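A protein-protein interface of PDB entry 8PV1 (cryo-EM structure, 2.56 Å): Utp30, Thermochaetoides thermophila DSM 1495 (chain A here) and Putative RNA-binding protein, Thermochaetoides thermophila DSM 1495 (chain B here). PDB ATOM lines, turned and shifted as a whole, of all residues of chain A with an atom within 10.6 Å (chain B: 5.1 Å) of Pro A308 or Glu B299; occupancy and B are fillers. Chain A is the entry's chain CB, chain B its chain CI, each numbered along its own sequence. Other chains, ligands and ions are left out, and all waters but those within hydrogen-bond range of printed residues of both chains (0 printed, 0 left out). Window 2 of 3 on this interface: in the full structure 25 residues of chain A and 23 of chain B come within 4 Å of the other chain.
The backbone carbonyl oxygen (O) of Leu B297 is in hydrogen-bond range of the indole nitrogen (NE1) of Trp B302 (3.1 Å).
NE2 of Gln B301 sits close to N of Ser B298 (2.9 Å).
N of Leu B297 is in hydrogen-bond range of O of Lys A305 (3.3 Å).
The side-chain carboxylate of Glu B299 sits close to the backbone carbonyl oxygen of Val A307 (3.2 Å).
Of the printed residues of chain B, Leu A299 touches Trp B302 (3.4 Å).
Of the printed residues of chain B, Trp A300 touches Trp B302 and Pro B335.
Of the printed residues of chain B, Lys A305 touches Leu B297 and Trp B302.
Pro A308 touches just one residue of chain B: Glu B299 (3.6 Å).
Of the printed residues of chain A, Leu B297 touches Lys A305 (3.1 Å) and Val A307 (3.5 Å).
Of chain A, only Val A307 (3.2 Å) and Pro A308 (3.6 Å) come within 4 Å of Glu B299.
No residue of chain A comes within 4 Å of Ser B300.
Of the printed residues of chain A, Trp B302 touches Leu A299, Trp A300 and Lys A305.
No residue of chain A comes within 4 Å of Gln B303.
The nearest residue of chain B that does not touch Pro A308 is Ser B298 (4.7 Å).
The nearest printed residue of chain A that does not touch Leu B297 is Val A306 (4.2 Å).
Among the printed residues, pairs that only touch across the chains: Leu A299 with Trp B302, Trp A300 with Trp B302, Trp A300 with Pro B335, Lys A305 with Trp B302, Val A307 with Leu B297, Val A307 with Ser B298 and Pro A308 with Glu B299.
Hydrophobic or aromatic side chains of chain A that line the printed part of chain B: Leu A299, Trp A300 and Val A307.
Of the 8 printed residues of chain B, 5 touch a printed residue of chain A.
Hydrophobic or aromatic side chains of chain B within 4 Å of the printed part of chain A: Trp B302 and Pro B335.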
ATOM      1  N   LEU A 299     -10.532 -11.082   7.667  1.00  0.00           N
ATOM      2  CA  LEU A 299     -10.740 -11.226   9.102  1.00  0.00           C
ATOM      3  C   LEU A 299     -11.375 -12.559   9.480  1.00  0.00           C
ATOM      4  O   LEU A 299     -11.680 -12.776  10.656  1.00  0.00           O
ATOM      5  CB  LEU A 299     -11.596 -10.074   9.632  1.00  0.00           C
ATOM      6  CG  LEU A 299     -11.075  -8.667   9.341  1.00  0.00           C
ATOM      7  CD1 LEU A 299     -12.096  -7.623   9.760  1.00  0.00           C
ATOM      8  CD2 LEU A 299      -9.744  -8.435  10.040  1.00  0.00           C
ATOM      9  N   TRP A 300     -11.580 -13.452   8.518  1.00  0.00           N
ATOM     10  CA  TRP A 300     -12.206 -14.741   8.763  1.00  0.00           C
ATOM     11  C   TRP A 300     -11.184 -15.857   8.598  1.00  0.00           C
ATOM     12  O   TRP A 300     -10.198 -15.715   7.871  1.00  0.00           O
ATOM     13  CB  TRP A 300     -13.387 -14.969   7.813  1.00  0.00           C
ATOM     14  CG  TRP A 300     -13.138 -14.491   6.413  1.00  0.00           C
ATOM     15  CD1 TRP A 300     -12.642 -15.221   5.374  1.00  0.00           C
ATOM     16  CD2 TRP A 300     -13.360 -13.170   5.905  1.00  0.00           C
ATOM     17  NE1 TRP A 300     -12.550 -14.439   4.248  1.00  0.00           N
ATOM     18  CE2 TRP A 300     -12.982 -13.174   4.550  1.00  0.00           C
ATOM     19  CE3 TRP A 300     -13.840 -11.984   6.467  1.00  0.00           C
ATOM     20  CZ2 TRP A 300     -13.073 -12.040   3.747  1.00  0.00           C
ATOM     21  CZ3 TRP A 300     -13.930 -10.861   5.669  1.00  0.00           C
ATOM     22  CH2 TRP A 300     -13.547 -10.896   4.326  1.00  0.00           C
ATOM     23  N   GLU A 303     -14.064 -19.582   4.443  1.00  0.00           N
ATOM     24  CA  GLU A 303     -15.365 -19.202   3.908  1.00  0.00           C
ATOM     25  C   GLU A 303     -16.525 -19.771   4.714  1.00  0.00           C
ATOM     26  O   GLU A 303     -17.667 -19.341   4.516  1.00  0.00           O
ATOM     27  CB  GLU A 303     -15.487 -19.649   2.449  1.00  0.00           C
ATOM     28  CG  GLU A 303     -15.578 -21.157   2.258  1.00  0.00           C
ATOM     29  CD  GLU A 303     -14.222 -21.816   2.075  1.00  0.00           C
ATOM     30  OE1 GLU A 303     -13.195 -21.158   2.341  1.00  0.00           O
ATOM     31  OE2 GLU A 303     -14.186 -22.993   1.662  1.00  0.00           O
ATOM     32  N   SER A 304     -16.263 -20.727   5.609  1.00  0.00           N
ATOM     33  CA  SER A 304     -17.339 -21.306   6.407  1.00  0.00           C
ATOM     34  C   SER A 304     -17.847 -20.329   7.459  1.00  0.00           C
ATOM     35  O   SER A 304     -18.999 -20.431   7.894  1.00  0.00           O
ATOM     36  CB  SER A 304     -16.866 -22.600   7.070  1.00  0.00           C
ATOM     37  OG  SER A 304     -15.850 -22.344   8.022  1.00  0.00           O
ATOM     38  N   LYS A 305     -17.004 -19.385   7.884  1.00  0.00           N
ATOM     39  CA  LYS A 305     -17.445 -18.378   8.844  1.00  0.00           C
ATOM     40  C   LYS A 305     -18.430 -17.406   8.208  1.00  0.00           C
ATOM     41  O   LYS A 305     -19.336 -16.898   8.880  1.00  0.00           O
ATOM     42  CB  LYS A 305     -16.239 -17.631   9.412  1.00  0.00           C
ATOM     43  CG  LYS A 305     -15.258 -18.520  10.157  1.00  0.00           C
ATOM     44  CD  LYS A 305     -15.878 -19.082  11.426  1.00  0.00           C
ATOM     45  CE  LYS A 305     -14.852 -19.825  12.265  1.00  0.00           C
ATOM     46  NZ  LYS A 305     -14.438 -21.107  11.632  1.00  0.00           N
ATOM     47  N   VAL A 306     -18.270 -17.132   6.916  1.00  0.00           N
ATOM     48  CA  VAL A 306     -19.190 -16.256   6.198  1.00  0.00           C
ATOM     49  C   VAL A 306     -20.433 -17.067   5.839  1.00  0.00           C
ATOM     50  O   VAL A 306     -20.346 -18.062   5.113  1.00  0.00           O
ATOM     51  CB  VAL A 306     -18.538 -15.654   4.951  1.00  0.00           C
ATOM     52  CG1 VAL A 306     -19.530 -14.773   4.208  1.00  0.00           C
ATOM     53  CG2 VAL A 306     -17.297 -14.863   5.333  1.00  0.00           C
ATOM     54  N   VAL A 307     -21.587 -16.646   6.344  1.00  0.00           N
ATOM     55  CA  VAL A 307     -22.843 -17.351   6.101  1.00  0.00           C
ATOM     56  C   VAL A 307     -23.878 -16.340   5.613  1.00  0.00           C
ATOM     57  O   VAL A 307     -23.870 -15.179   6.051  1.00  0.00           O
ATOM     58  CB  VAL A 307     -23.292 -18.118   7.362  1.00  0.00           C
ATOM     59  CG1 VAL A 307     -23.698 -17.175   8.496  1.00  0.00           C
ATOM     60  CG2 VAL A 307     -24.415 -19.102   7.049  1.00  0.00           C
ATOM     61  N   PRO A 308     -24.745 -16.705   4.654  1.00  0.00           N
ATOM     62  CA  PRO A 308     -25.837 -15.808   4.270  1.00  0.00           C
ATOM     63  C   PRO A 308     -27.169 -16.209   4.896  1.00  0.00           C
ATOM     64  O   PRO A 308     -27.881 -15.335   5.391  1.00  0.00           O
ATOM     65  CB  PRO A 308     -25.888 -15.946   2.744  1.00  0.00           C
ATOM     66  CG  PRO A 308     -25.115 -17.210   2.412  1.00  0.00           C
ATOM     67  CD  PRO A 308     -24.573 -17.796   3.682  1.00  0.00           C
ATOM     68  N   LEU B 297     -20.829 -15.804  11.642  1.00  0.00           N
ATOM     69  CA  LEU B 297     -21.682 -14.627  11.686  1.00  0.00           C
ATOM     70  C   LEU B 297     -22.084 -14.256  10.266  1.00  0.00           C
ATOM     71  O   LEU B 297     -21.417 -14.614   9.293  1.00  0.00           O
ATOM     72  CB  LEU B 297     -21.004 -13.423  12.367  1.00  0.00           C
ATOM     73  CG  LEU B 297     -20.981 -13.260  13.897  1.00  0.00           C
ATOM     74  CD1 LEU B 297     -22.389 -13.094  14.469  1.00  0.00           C
ATOM     75  CD2 LEU B 297     -20.215 -14.355  14.628  1.00  0.00           C
ATOM     76  N   SER B 298     -23.196 -13.536  10.158  1.00  0.00           N
ATOM     77  CA  SER B 298     -23.736 -13.160   8.863  1.00  0.00           C
ATOM     78  C   SER B 298     -23.063 -11.903   8.324  1.00  0.00           C
ATOM     79  O   SER B 298     -22.314 -11.210   9.027  1.00  0.00           O
ATOM     80  CB  SER B 298     -25.248 -12.949   8.949  1.00  0.00           C
ATOM     81  OG  SER B 298     -25.895 -14.112   9.438  1.00  0.00           O
ATOM     82  N   GLU B 299     -23.368 -11.604   7.058  1.00  0.00           N
ATOM     83  CA  GLU B 299     -22.581 -10.638   6.298  1.00  0.00           C
ATOM     84  C   GLU B 299     -22.764  -9.214   6.813  1.00  0.00           C
ATOM     85  O   GLU B 299     -21.831  -8.411   6.751  1.00  0.00           O
ATOM     86  CB  GLU B 299     -22.924 -10.744   4.807  1.00  0.00           C
ATOM     87  CG  GLU B 299     -24.322 -10.279   4.395  1.00  0.00           C
ATOM     88  CD  GLU B 299     -25.391 -11.352   4.551  1.00  0.00           C
ATOM     89  OE1 GLU B 299     -25.147 -12.360   5.247  1.00  0.00           O
ATOM     90  OE2 GLU B 299     -26.481 -11.186   3.962  1.00  0.00           O
ATOM     91  N   SER B 300     -23.941  -8.889   7.356  1.00  0.00           N
ATOM     92  CA  SER B 300     -24.188  -7.525   7.825  1.00  0.00           C
ATOM     93  C   SER B 300     -23.346  -7.200   9.057  1.00  0.00           C
ATOM     94  O   SER B 300     -22.688  -6.150   9.126  1.00  0.00           O
ATOM     95  CB  SER B 300     -25.677  -7.335   8.119  1.00  0.00           C
ATOM     96  OG  SER B 300     -25.941  -6.023   8.583  1.00  0.00           O
ATOM     97  N   GLN B 301     -23.332  -8.100  10.041  1.00  0.00           N
ATOM     98  CA  GLN B 301     -22.485  -7.856  11.200  1.00  0.00           C
ATOM     99  C   GLN B 301     -21.009  -8.082  10.888  1.00  0.00           C
ATOM    100  O   GLN B 301     -20.148  -7.510  11.569  1.00  0.00           O
ATOM    101  CB  GLN B 301     -22.962  -8.682  12.399  1.00  0.00           C
ATOM    102  CG  GLN B 301     -22.978 -10.188  12.252  1.00  0.00           C
ATOM    103  CD  GLN B 301     -24.312 -10.686  11.716  1.00  0.00           C
ATOM    104  OE1 GLN B 301     -25.038  -9.952  11.047  1.00  0.00           O
ATOM    105  NE2 GLN B 301     -24.678 -11.905  12.089  1.00  0.00           N
ATOM    106  N   TRP B 302     -20.683  -8.838   9.831  1.00  0.00           N
ATOM    107  CA  TRP B 302     -19.300  -8.804   9.354  1.00  0.00           C
ATOM    108  C   TRP B 302     -18.931  -7.437   8.780  1.00  0.00           C
ATOM    109  O   TRP B 302     -17.795  -6.978   8.948  1.00  0.00           O
ATOM    110  CB  TRP B 302     -19.014  -9.907   8.333  1.00  0.00           C
ATOM    111  CG  TRP B 302     -18.633 -11.209   8.960  1.00  0.00           C
ATOM    112  CD1 TRP B 302     -19.459 -12.211   9.358  1.00  0.00           C
ATOM    113  CD2 TRP B 302     -17.313 -11.600   9.350  1.00  0.00           C
ATOM    114  NE1 TRP B 302     -18.730 -13.233   9.918  1.00  0.00           N
ATOM    115  CE2 TRP B 302     -17.409 -12.874   9.935  1.00  0.00           C
ATOM    116  CE3 TRP B 302     -16.054 -11.001   9.243  1.00  0.00           C
ATOM    117  CZ2 TRP B 302     -16.297 -13.563  10.412  1.00  0.00           C
ATOM    118  CZ3 TRP B 302     -14.953 -11.683   9.719  1.00  0.00           C
ATOM    119  CH2 TRP B 302     -15.080 -12.951  10.294  1.00  0.00           C
ATOM    120  N   GLN B 303     -19.869  -6.774   8.090  1.00  0.00           N
ATOM    121  CA  GLN B 303     -19.622  -5.399   7.653  1.00  0.00           C
ATOM    122  C   GLN B 303     -19.409  -4.470   8.840  1.00  0.00           C
ATOM    123  O   GLN B 303     -18.528  -3.598   8.805  1.00  0.00           O
ATOM    124  CB  GLN B 303     -20.768  -4.873   6.782  1.00  0.00           C
ATOM    125  CG  GLN B 303     -21.020  -5.634   5.498  1.00  0.00           C
ATOM    126  CD  GLN B 303     -19.861  -5.534   4.527  1.00  0.00           C
ATOM    127  OE1 GLN B 303     -19.520  -6.501   3.849  1.00  0.00           O
ATOM    128  NE2 GLN B 303     -19.257  -4.353   4.448  1.00  0.00           N
ATOM    129  N   PRO B 335     -16.686  -8.837   1.879  1.00  0.00           N
ATOM    130  CA  PRO B 335     -17.434 -10.075   1.626  1.00  0.00           C
ATOM    131  C   PRO B 335     -18.634  -9.878   0.701  1.00  0.00           C
ATOM    132  O   PRO B 335     -19.701 -10.423   0.988  1.00  0.00           O
ATOM    133  CB  PRO B 335     -17.906 -10.491   3.023  1.00  0.00           C
ATOM    134  CG  PRO B 335     -16.938  -9.857   3.951  1.00  0.00           C
ATOM    135  CD  PRO B 335     -16.591  -8.545   3.321  1.00  0.00           C
